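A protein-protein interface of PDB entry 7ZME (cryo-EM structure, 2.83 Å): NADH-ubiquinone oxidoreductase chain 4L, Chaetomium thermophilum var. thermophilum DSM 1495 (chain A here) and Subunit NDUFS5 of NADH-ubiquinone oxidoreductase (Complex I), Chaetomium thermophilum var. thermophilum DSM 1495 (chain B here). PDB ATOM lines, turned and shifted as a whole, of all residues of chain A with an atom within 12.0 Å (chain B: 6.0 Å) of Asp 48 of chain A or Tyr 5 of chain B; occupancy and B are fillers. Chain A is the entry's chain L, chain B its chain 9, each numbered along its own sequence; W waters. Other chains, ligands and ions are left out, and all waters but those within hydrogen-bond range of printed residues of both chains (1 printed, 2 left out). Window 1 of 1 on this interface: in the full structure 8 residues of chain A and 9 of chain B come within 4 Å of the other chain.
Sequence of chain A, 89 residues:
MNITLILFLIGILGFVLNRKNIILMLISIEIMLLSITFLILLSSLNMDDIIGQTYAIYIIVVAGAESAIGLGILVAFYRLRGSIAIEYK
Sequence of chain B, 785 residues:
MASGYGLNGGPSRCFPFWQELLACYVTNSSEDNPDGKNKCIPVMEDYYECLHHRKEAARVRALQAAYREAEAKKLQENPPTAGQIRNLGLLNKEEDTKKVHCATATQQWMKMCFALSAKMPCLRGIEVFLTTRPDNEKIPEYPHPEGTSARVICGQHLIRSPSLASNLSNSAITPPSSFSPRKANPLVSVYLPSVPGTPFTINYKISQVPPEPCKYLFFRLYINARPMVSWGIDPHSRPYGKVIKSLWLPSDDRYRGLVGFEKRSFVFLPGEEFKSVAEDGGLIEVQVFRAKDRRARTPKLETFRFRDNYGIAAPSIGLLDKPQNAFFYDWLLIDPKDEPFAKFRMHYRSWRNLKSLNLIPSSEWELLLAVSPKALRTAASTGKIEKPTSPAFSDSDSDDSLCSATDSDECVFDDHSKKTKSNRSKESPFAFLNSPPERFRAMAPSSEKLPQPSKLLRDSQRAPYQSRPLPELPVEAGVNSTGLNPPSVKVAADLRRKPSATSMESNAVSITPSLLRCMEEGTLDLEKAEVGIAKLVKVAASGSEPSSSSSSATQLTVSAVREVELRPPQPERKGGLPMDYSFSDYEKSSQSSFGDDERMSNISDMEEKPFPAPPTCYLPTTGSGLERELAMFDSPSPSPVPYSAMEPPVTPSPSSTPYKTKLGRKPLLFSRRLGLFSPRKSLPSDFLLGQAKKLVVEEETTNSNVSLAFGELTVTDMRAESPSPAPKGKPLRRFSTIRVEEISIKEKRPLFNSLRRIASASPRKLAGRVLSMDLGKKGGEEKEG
The backbone carbonyl oxygen of Tyr 5 of chain B lies within hydrogen-bond range of the backbone NH of Ile 50 of chain A, 3.1 Å away. The backbone carbonyl oxygen of Asn 46 of chain A sits at hydrogen-bond distance from the guanidinium group of Arg 13 of chain B, at 2.6 Å. The backbone NH of Met 1 of chain B is in hydrogen-bond range of the backbone carbonyl oxygen of Met 47 of chain A (2.6 Å). The side-chain carboxylate (OD1) of Asp 49 of chain A sits at hydrogen-bond distance from the backbone NH (N) of Met 1 of chain B (2.9 Å). OD1 of Asp 49 of chain A sits at hydrogen-bond distance from OG of Ser 3 of chain B (3.1 Å).
Printed residues of chain A that touch a printed residue of chain B: Leu 45, Asn 46, Met 47, Asp 48, Asp 49, Ile 50, Ile 51 and Gln 53. Among the printed residues, 19 pairs touch across the chains. Among the printed residues, no Asp or Glu carboxylate lies within 4 Å of a Lys or Arg side-chain nitrogen of the other chain.
Water W1 lies within hydrogen-bond range of the guanidinium group of Arg 13 of chain B (3.0 Å), the backbone carbonyl oxygen of Asn 46 of chain A (3.2 Å) and the backbone carbonyl oxygen of Leu 45 of chain A (3.2 Å).
Among the printed residues, merely in contact across the chains: Leu 45 of chain A with Leu 7 of chain B (3.8 Å), Met 47 of chain A with Arg 13 of chain B (3.9 Å), Asp 48 of chain A with Tyr 5 of chain B (3.9 Å), Asp 48 of chain A with Gly 6 of chain B (3.1 Å), Asp 48 of chain A with Leu 7 of chain B (3.6 Å), Asp 48 of chain A with Pro 11 of chain B (3.8 Å), Asp 48 of chain A with Ser 12 of chain B (3.4 Å), Asp 48 of chain A with Arg 13 of chain B (3.6 Å), Asp 49 of chain A with Tyr 5 of chain B (3.96 Å), Asp 49 of chain A with Leu 7 of chain B (3.8 Å), Ile 50 of chain A with Gly 6 of chain B (3.5 Å), Ile 50 of chain A with Leu 7 of chain B (3.9 Å), Ile 51 of chain A with Ser 3 of chain B (3.4 Å) and Gln 53 of chain A with Leu 7 of chain B (3.4 Å).
The backbone carbonyl oxygen (O) of Met 1 of chain B is in hydrogen-bond range of the side-chain hydroxyl (OG) of Ser 12 of chain B (2.6 Å). The guanidinium group (NH2) of Arg 13 of chain B lies within hydrogen-bond range of the side-chain sulfur (SG) of Cys 14 of chain B (3.4 Å). The backbone NH (N) of Phe 15 of chain B lies within hydrogen-bond range of the backbone carbonyl oxygen (O) of Met 1 of chain B (3.5 Å). The backbone carbonyl oxygen (O) of Leu 42 of chain A sits close to the side-chain amide oxygen (OD1) of Asn 46 of chain A (3.1 Å). The backbone NH (N) of Gly 4 of chain B sits at hydrogen-bond distance from the side-chain hydroxyl (OG) of Ser 12 of chain B (3.0 Å). The backbone carbonyl oxygen of Ile 50 of chain A is in hydrogen-bond range of the side-chain hydroxyl of Thr 54 of chain A (2.8 Å).
Of the printed residues of chain B, Asp 48 of chain A touches Tyr 5, Gly 6, Leu 7, Pro 11, Ser 12 and Arg 13. Tyr 5 of chain B touches three residues of chain A. Met 1 of chain B touches just these residues of chain A: Met 47 and Asp 49. No residue of chain A comes within 4 Å of Gly 4 of chain B. Of the printed residues of chain A, Gly 6 of chain B touches Asp 48 (3.1 Å) and Ile 50 (3.5 Å). Leu 7 of chain B touches five residues of chain A. No residue of chain A comes within 4 Å of Gly 10 of chain B. Ser 12 of chain B touches one residue of chain A. Of the printed residues of chain A, Arg 13 of chain B touches Asn 46 (2.6 Å), Met 47 (3.9 Å) and Asp 48 (3.6 Å). Of the printed residues of chain B, Asn 46 of chain A touches Arg 13 (2.6 Å). Printed residues of chain B within 4 Å of Ile 50 of chain A: Tyr 5, Gly 6 and Leu 7. Of the printed residues of chain B, Met 47 of chain A touches Met 1 (2.6 Å) and Arg 13 (3.9 Å). The nearest printed residue of chain B that does not touch Met 47 of chain A is Ser 12 of chain B (4.5 Å).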
ATOM      1  N   LEU A  39     -24.829 -31.650   5.030  1.00  0.00           N
ATOM      2  CA  LEU A  39     -23.472 -31.114   5.092  1.00  0.00           C
ATOM      3  C   LEU A  39     -23.442 -29.768   5.800  1.00  0.00           C
ATOM      4  O   LEU A  39     -22.534 -29.495   6.592  1.00  0.00           O
ATOM      5  CB  LEU A  39     -22.889 -30.989   3.685  1.00  0.00           C
ATOM      6  CG  LEU A  39     -21.553 -30.253   3.607  1.00  0.00           C
ATOM      7  CD1 LEU A  39     -20.439 -31.107   4.169  1.00  0.00           C
ATOM      8  CD2 LEU A  39     -21.248 -29.827   2.186  1.00  0.00           C
ATOM      9  N   ILE A  40     -24.427 -28.912   5.522  1.00  0.00           N
ATOM     10  CA  ILE A  40     -24.490 -27.601   6.160  1.00  0.00           C
ATOM     11  C   ILE A  40     -24.733 -27.745   7.657  1.00  0.00           C
ATOM     12  O   ILE A  40     -24.193 -26.982   8.464  1.00  0.00           O
ATOM     13  CB  ILE A  40     -25.572 -26.738   5.484  1.00  0.00           C
ATOM     14  CG1 ILE A  40     -25.261 -26.578   3.996  1.00  0.00           C
ATOM     15  CG2 ILE A  40     -25.680 -25.379   6.139  1.00  0.00           C
ATOM     16  CD1 ILE A  40     -26.415 -26.052   3.185  1.00  0.00           C
ATOM     17  N   LEU A  41     -25.492 -28.742   8.076  1.00  0.00           N
ATOM     18  CA  LEU A  41     -25.806 -28.946   9.517  1.00  0.00           C
ATOM     19  C   LEU A  41     -24.565 -29.376  10.288  1.00  0.00           C
ATOM     20  O   LEU A  41     -24.336 -28.829  11.374  1.00  0.00           O
ATOM     21  CB  LEU A  41     -26.977 -29.911   9.697  1.00  0.00           C
ATOM     22  CG  LEU A  41     -28.343 -29.305   9.381  1.00  0.00           C
ATOM     23  CD1 LEU A  41     -29.425 -30.367   9.331  1.00  0.00           C
ATOM     24  CD2 LEU A  41     -28.701 -28.224  10.385  1.00  0.00           C
ATOM     25  N   LEU A  42     -23.839 -30.362   9.783  1.00  0.00           N
ATOM     26  CA  LEU A  42     -22.609 -30.846  10.458  1.00  0.00           C
ATOM     27  C   LEU A  42     -21.563 -29.731  10.538  1.00  0.00           C
ATOM     28  O   LEU A  42     -20.908 -29.644  11.570  1.00  0.00           O
ATOM     29  CB  LEU A  42     -22.101 -32.068   9.690  1.00  0.00           C
ATOM     30  CG  LEU A  42     -23.064 -33.249   9.617  1.00  0.00           C
ATOM     31  CD1 LEU A  42     -22.472 -34.376   8.792  1.00  0.00           C
ATOM     32  CD2 LEU A  42     -23.413 -33.741  11.005  1.00  0.00           C
ATOM     33  N   SER A  43     -21.400 -28.931   9.488  1.00  0.00           N
ATOM     34  CA  SER A  43     -20.444 -27.794   9.461  1.00  0.00           C
ATOM     35  C   SER A  43     -20.838 -26.739  10.478  1.00  0.00           C
ATOM     36  O   SER A  43     -19.958 -26.201  11.149  1.00  0.00           O
ATOM     37  CB  SER A  43     -20.405 -27.210   8.097  1.00  0.00           C
ATOM     38  OG  SER A  43     -20.130 -28.223   7.146  1.00  0.00           O
ATOM     39  N   SER A  44     -22.126 -26.409  10.528  1.00  0.00           N
ATOM     40  CA  SER A  44     -22.659 -25.441  11.516  1.00  0.00           C
ATOM     41  C   SER A  44     -22.240 -25.861  12.927  1.00  0.00           C
ATOM     42  O   SER A  44     -21.858 -24.976  13.706  1.00  0.00           O
ATOM     43  CB  SER A  44     -24.141 -25.346  11.383  1.00  0.00           C
ATOM     44  OG  SER A  44     -24.492 -25.124  10.037  1.00  0.00           O
ATOM     45  N   LEU A  45     -22.411 -27.137  13.264  1.00  0.00           N
ATOM     46  CA  LEU A  45     -22.036 -27.650  14.602  1.00  0.00           C
ATOM     47  C   LEU A  45     -20.538 -27.472  14.840  1.00  0.00           C
ATOM     48  O   LEU A  45     -20.174 -27.139  15.971  1.00  0.00           O
ATOM     49  CB  LEU A  45     -22.452 -29.120  14.682  1.00  0.00           C
ATOM     50  CG  LEU A  45     -22.190 -29.838  16.003  1.00  0.00           C
ATOM     51  CD1 LEU A  45     -22.965 -29.188  17.137  1.00  0.00           C
ATOM     52  CD2 LEU A  45     -22.555 -31.306  15.885  1.00  0.00           C
ATOM     53  N   ASN A  46     -19.708 -27.657  13.818  1.00  0.00           N
ATOM     54  CA  ASN A  46     -18.238 -27.602  14.015  1.00  0.00           C
ATOM     55  C   ASN A  46     -17.772 -26.148  14.070  1.00  0.00           C
ATOM     56  O   ASN A  46     -16.701 -25.922  14.632  1.00  0.00           O
ATOM     57  CB  ASN A  46     -17.491 -28.255  12.853  1.00  0.00           C
ATOM     58  CG  ASN A  46     -17.903 -29.679  12.557  1.00  0.00           C
ATOM     59  OD1 ASN A  46     -17.811 -30.126  11.417  1.00  0.00           O
ATOM     60  ND2 ASN A  46     -18.363 -30.398  13.565  1.00  0.00           N
ATOM     61  N   MET A  47     -18.555 -25.205  13.530  1.00  0.00           N
ATOM     62  CA  MET A  47     -18.189 -23.768  13.589  1.00  0.00           C
ATOM     63  C   MET A  47     -19.054 -22.968  14.570  1.00  0.00           C
ATOM     64  O   MET A  47     -18.898 -21.743  14.580  1.00  0.00           O
ATOM     65  CB  MET A  47     -18.279 -23.159  12.190  1.00  0.00           C
ATOM     66  CG  MET A  47     -17.554 -23.975  11.135  1.00  0.00           C
ATOM     67  SD  MET A  47     -17.669 -23.310   9.454  1.00  0.00           S
ATOM     68  CE  MET A  47     -19.424 -23.461   9.122  1.00  0.00           C
ATOM     69  N   ASP A  48     -19.893 -23.619  15.379  1.00  0.00           N
ATOM     70  CA  ASP A  48     -20.766 -22.936  16.383  1.00  0.00           C
ATOM     71  C   ASP A  48     -21.661 -21.895  15.703  1.00  0.00           C
ATOM     72  O   ASP A  48     -21.738 -20.782  16.202  1.00  0.00           O
ATOM     73  CB  ASP A  48     -19.932 -22.336  17.513  1.00  0.00           C
ATOM     74  CG  ASP A  48     -20.673 -22.249  18.826  1.00  0.00           C
ATOM     75  OD1 ASP A  48     -21.259 -23.273  19.219  1.00  0.00           O
ATOM     76  OD2 ASP A  48     -20.658 -21.161  19.432  1.00  0.00           O
ATOM     77  N   ASP A  49     -22.287 -22.245  14.586  1.00  0.00           N
ATOM     78  CA  ASP A  49     -23.074 -21.270  13.794  1.00  0.00           C
ATOM     79  C   ASP A  49     -24.559 -21.621  13.773  1.00  0.00           C
ATOM     80  O   ASP A  49     -24.904 -22.659  13.198  1.00  0.00           O
ATOM     81  CB  ASP A  49     -22.675 -21.395  12.335  1.00  0.00           C
ATOM     82  CG  ASP A  49     -21.497 -20.544  11.926  1.00  0.00           C
ATOM     83  OD1 ASP A  49     -21.436 -19.381  12.356  1.00  0.00           O
ATOM     84  OD2 ASP A  49     -20.670 -21.056  11.162  1.00  0.00           O
ATOM     85  N   ILE A  50     -25.404 -20.775  14.335  1.00  0.00           N
ATOM     86  CA  ILE A  50     -26.841 -20.987  14.277  1.00  0.00           C
ATOM     87  C   ILE A  50     -27.399 -20.581  12.921  1.00  0.00           C
ATOM     88  O   ILE A  50     -28.559 -20.877  12.614  1.00  0.00           O
ATOM     89  CB  ILE A  50     -27.519 -20.245  15.448  1.00  0.00           C
ATOM     90  CG1 ILE A  50     -28.877 -20.867  15.760  1.00  0.00           C
ATOM     91  CG2 ILE A  50     -27.666 -18.773  15.145  1.00  0.00           C
ATOM     92  CD1 ILE A  50     -28.782 -22.279  16.277  1.00  0.00           C
ATOM     93  N   ILE A  51     -26.579 -19.933  12.092  1.00  0.00           N
ATOM     94  CA  ILE A  51     -27.014 -19.505  10.767  1.00  0.00           C
ATOM     95  C   ILE A  51     -27.133 -20.692   9.824  1.00  0.00           C
ATOM     96  O   ILE A  51     -28.031 -20.740   8.977  1.00  0.00           O
ATOM     97  CB  ILE A  51     -26.057 -18.428  10.225  1.00  0.00           C
ATOM     98  CG1 ILE A  51     -26.226 -17.158  11.042  1.00  0.00           C
ATOM     99  CG2 ILE A  51     -26.300 -18.147   8.753  1.00  0.00           C
ATOM    100  CD1 ILE A  51     -27.627 -16.697  11.085  1.00  0.00           C
ATOM    101  N   GLY A  52     -26.236 -21.668   9.950  1.00  0.00           N
ATOM    102  CA  GLY A  52     -26.329 -22.840   9.105  1.00  0.00           C
ATOM    103  C   GLY A  52     -27.495 -23.742   9.433  1.00  0.00           C
ATOM    104  O   GLY A  52     -27.947 -24.492   8.564  1.00  0.00           O
ATOM    105  N   GLN A  53     -27.982 -23.705  10.674  1.00  0.00           N
ATOM    106  CA  GLN A  53     -29.245 -24.364  10.984  1.00  0.00           C
ATOM    107  C   GLN A  53     -30.410 -23.581  10.410  1.00  0.00           C
ATOM    108  O   GLN A  53     -31.394 -24.165   9.945  1.00  0.00           O
ATOM    109  CB  GLN A  53     -29.405 -24.521  12.493  1.00  0.00           C
ATOM    110  CG  GLN A  53     -28.624 -25.669  13.091  1.00  0.00           C
ATOM    111  CD  GLN A  53     -28.992 -25.914  14.532  1.00  0.00           C
ATOM    112  OE1 GLN A  53     -30.167 -26.016  14.873  1.00  0.00           O
ATOM    113  NE2 GLN A  53     -27.990 -25.996  15.391  1.00  0.00           N
ATOM    114  N   THR A  54     -30.321 -22.253  10.450  1.00  0.00           N
ATOM    115  CA  THR A  54     -31.312 -21.410   9.794  1.00  0.00           C
ATOM    116  C   THR A  54     -31.279 -21.603   8.285  1.00  0.00           C
ATOM    117  O   THR A  54     -32.329 -21.624   7.634  1.00  0.00           O
ATOM    118  CB  THR A  54     -31.061 -19.948  10.157  1.00  0.00           C
ATOM    119  OG1 THR A  54     -30.911 -19.834  11.577  1.00  0.00           O
ATOM    120  CG2 THR A  54     -32.210 -19.067   9.694  1.00  0.00           C
ATOM    121  N   TYR A  55     -30.081 -21.737   7.715  1.00  0.00           N
ATOM    122  CA  TYR A  55     -29.955 -22.003   6.288  1.00  0.00           C
ATOM    123  C   TYR A  55     -30.560 -23.355   5.939  1.00  0.00           C
ATOM    124  O   TYR A  55     -31.264 -23.491   4.933  1.00  0.00           O
ATOM    125  CB  TYR A  55     -28.481 -21.948   5.885  1.00  0.00           C
ATOM    126  CG  TYR A  55     -28.199 -22.016   4.398  1.00  0.00           C
ATOM    127  CD1 TYR A  55     -29.200 -21.786   3.466  1.00  0.00           C
ATOM    128  CD2 TYR A  55     -26.918 -22.264   3.930  1.00  0.00           C
ATOM    129  CE1 TYR A  55     -28.941 -21.824   2.120  1.00  0.00           C
ATOM    130  CE2 TYR A  55     -26.649 -22.305   2.582  1.00  0.00           C
ATOM    131  CZ  TYR A  55     -27.667 -22.083   1.681  1.00  0.00           C
ATOM    132  OH  TYR A  55     -27.413 -22.120   0.333  1.00  0.00           O
ATOM    133  N   MET B   1     -18.848 -19.247  13.711  1.00  0.00           N
ATOM    134  CA  MET B   1     -18.042 -18.628  12.667  1.00  0.00           C
ATOM    135  C   MET B   1     -18.349 -17.148  12.513  1.00  0.00           C
ATOM    136  O   MET B   1     -18.463 -16.422  13.498  1.00  0.00           O
ATOM    137  CB  MET B   1     -18.256 -19.342  11.336  1.00  0.00           C
ATOM    138  N   SER B   3     -20.848 -15.289  11.629  1.00  0.00           N
ATOM    139  CA  SER B   3     -22.129 -14.640  11.873  1.00  0.00           C
ATOM    140  C   SER B   3     -22.172 -13.877  13.193  1.00  0.00           C
ATOM    141  O   SER B   3     -22.689 -12.757  13.239  1.00  0.00           O
ATOM    142  CB  SER B   3     -23.257 -15.675  11.834  1.00  0.00           C
ATOM    143  OG  SER B   3     -23.028 -16.751  12.731  1.00  0.00           O
ATOM    144  N   GLY B   4     -21.635 -14.447  14.263  1.00  0.00           N
ATOM    145  CA  GLY B   4     -21.732 -13.849  15.573  1.00  0.00           C
ATOM    146  C   GLY B   4     -22.851 -14.375  16.438  1.00  0.00           C
ATOM    147  O   GLY B   4     -23.096 -13.812  17.508  1.00  0.00           O
ATOM    148  N   TYR B   5     -23.558 -15.383  15.938  1.00  0.00           N
ATOM    149  CA  TYR B   5     -24.720 -15.964  16.644  1.00  0.00           C
ATOM    150  C   TYR B   5     -24.469 -17.465  16.725  1.00  0.00           C
ATOM    151  O   TYR B   5     -24.542 -18.134  15.708  1.00  0.00           O
ATOM    152  CB  TYR B   5     -26.001 -15.579  15.907  1.00  0.00           C
ATOM    153  CG  TYR B   5     -26.159 -14.094  15.718  1.00  0.00           C
ATOM    154  CD1 TYR B   5     -25.720 -13.472  14.562  1.00  0.00           C
ATOM    155  CD2 TYR B   5     -26.703 -13.302  16.713  1.00  0.00           C
ATOM    156  CE1 TYR B   5     -25.826 -12.104  14.393  1.00  0.00           C
ATOM    157  CE2 TYR B   5     -26.827 -11.934  16.555  1.00  0.00           C
ATOM    158  CZ  TYR B   5     -26.384 -11.334  15.392  1.00  0.00           C
ATOM    159  OH  TYR B   5     -26.496  -9.985  15.218  1.00  0.00           O
ATOM    160  N   GLY B   6     -24.105 -17.952  17.898  1.00  0.00           N
ATOM    161  CA  GLY B   6     -23.791 -19.370  18.108  1.00  0.00           C
ATOM    162  C   GLY B   6     -24.962 -20.225  18.532  1.00  0.00           C
ATOM    163  O   GLY B   6     -26.078 -19.704  18.633  1.00  0.00           O
ATOM    164  N   LEU B   7     -24.697 -21.481  18.870  1.00  0.00           N
ATOM    165  CA  LEU B   7     -25.752 -22.478  19.196  1.00  0.00           C
ATOM    166  C   LEU B   7     -26.526 -22.211  20.495  1.00  0.00           C
ATOM    167  O   LEU B   7     -27.703 -22.604  20.546  1.00  0.00           O
ATOM    168  CB  LEU B   7     -25.134 -23.874  19.117  1.00  0.00           C
ATOM    169  CG  LEU B   7     -24.435 -24.184  17.797  1.00  0.00           C
ATOM    170  CD1 LEU B   7     -23.726 -25.524  17.849  1.00  0.00           C
ATOM    171  CD2 LEU B   7     -25.417 -24.144  16.640  1.00  0.00           C
ATOM    172  N   ASN B   8     -25.906 -21.596  21.508  1.00  0.00           N
ATOM    173  CA  ASN B   8     -26.565 -21.453  22.839  1.00  0.00           C
ATOM    174  C   ASN B   8     -27.254 -20.106  23.059  1.00  0.00           C
ATOM    175  O   ASN B   8     -27.694 -19.870  24.186  1.00  0.00           O
ATOM    176  CB  ASN B   8     -25.632 -21.814  23.995  1.00  0.00           C
ATOM    177  CG  ASN B   8     -24.475 -20.863  24.217  1.00  0.00           C
ATOM    178  OD1 ASN B   8     -24.662 -19.717  24.617  1.00  0.00           O
ATOM    179  ND2 ASN B   8     -23.261 -21.347  24.013  1.00  0.00           N
ATOM    180  N   GLY B  10     -25.593 -17.458  22.722  1.00  0.00           N
ATOM    181  CA  GLY B  10     -24.409 -16.609  22.871  1.00  0.00           C
ATOM    182  C   GLY B  10     -23.738 -16.451  21.524  1.00  0.00           C
ATOM    183  O   GLY B  10     -24.269 -16.953  20.539  1.00  0.00           O
ATOM    184  N   PRO B  11     -22.590 -15.758  21.440  1.00  0.00           N
ATOM    185  CA  PRO B  11     -21.923 -15.494  20.168  1.00  0.00           C
ATOM    186  C   PRO B  11     -21.065 -16.651  19.644  1.00  0.00           C
ATOM    187  O   PRO B  11     -20.755 -17.526  20.406  1.00  0.00           O
ATOM    188  CB  PRO B  11     -21.002 -14.319  20.515  1.00  0.00           C
ATOM    189  CG  PRO B  11     -21.355 -13.900  21.921  1.00  0.00           C
ATOM    190  CD  PRO B  11     -21.901 -15.146  22.569  1.00  0.00           C
ATOM    191  N   SER B  12     -20.769 -16.668  18.354  1.00  0.00           N
ATOM    192  CA  SER B  12     -20.044 -17.780  17.688  1.00  0.00           C
ATOM    193  C   SER B  12     -18.574 -17.783  18.135  1.00  0.00           C
ATOM    194  O   SER B  12     -18.044 -16.704  18.384  1.00  0.00           O
ATOM    195  CB  SER B  12     -20.239 -17.737  16.189  1.00  0.00           C
ATOM    196  OG  SER B  12     -19.912 -16.467  15.660  1.00  0.00           O
ATOM    197  N   ARG B  13     -17.933 -18.943  18.200  1.00  0.00           N
ATOM    198  CA  ARG B  13     -16.522 -19.053  18.673  1.00  0.00           C
ATOM    199  C   ARG B  13     -15.549 -18.324  17.741  1.00  0.00           C
ATOM    200  O   ARG B  13     -14.567 -17.785  18.247  1.00  0.00           O
ATOM    201  CB  ARG B  13     -16.117 -20.503  18.951  1.00  0.00           C
ATOM    202  CG  ARG B  13     -16.431 -21.471  17.826  1.00  0.00           C
ATOM    203  CD  ARG B  13     -15.960 -22.867  18.168  1.00  0.00           C
ATOM    204  NE  ARG B  13     -15.831 -23.604  16.927  1.00  0.00           N
ATOM    205  CZ  ARG B  13     -14.718 -23.637  16.220  1.00  0.00           C
ATOM    206  NH1 ARG B  13     -14.669 -24.312  15.087  1.00  0.00           N
ATOM    207  NH2 ARG B  13     -13.651 -22.994  16.658  1.00  0.00           N
ATOM    208  N   CYS B  14     -15.772 -18.357  16.433  1.00  0.00           N
ATOM    209  CA  CYS B  14     -14.796 -17.746  15.496  1.00  0.00           C
ATOM    210  C   CYS B  14     -15.237 -16.335  15.117  1.00  0.00           C
ATOM    211  O   CYS B  14     -14.798 -15.867  14.076  1.00  0.00           O
ATOM    212  CB  CYS B  14     -14.625 -18.626  14.261  1.00  0.00           C
ATOM    213  SG  CYS B  14     -13.851 -20.207  14.650  1.00  0.00           S
ATOM    214  N   PHE B  15     -16.074 -15.704  15.932  1.00  0.00           N
ATOM    215  CA  PHE B  15     -16.461 -14.337  15.623  1.00  0.00           C
ATOM    216  C   PHE B  15     -15.379 -13.315  15.965  1.00  0.00           C
ATOM    217  O   PHE B  15     -15.180 -12.374  15.187  1.00  0.00           O
ATOM    218  CB  PHE B  15     -17.764 -13.977  16.333  1.00  0.00           C
ATOM    219  CG  PHE B  15     -18.398 -12.728  15.813  1.00  0.00           C
ATOM    220  CD1 PHE B  15     -18.662 -12.587  14.463  1.00  0.00           C
ATOM    221  CD2 PHE B  15     -18.712 -11.689  16.665  1.00  0.00           C
ATOM    222  CE1 PHE B  15     -19.233 -11.437  13.980  1.00  0.00           C
ATOM    223  CE2 PHE B  15     -19.286 -10.540  16.183  1.00  0.00           C
ATOM    224  CZ  PHE B  15     -19.550 -10.415  14.841  1.00  0.00           C
HETATM  225  O   HOH W   1     -17.801 -25.697  17.657  1.00  0.00           O
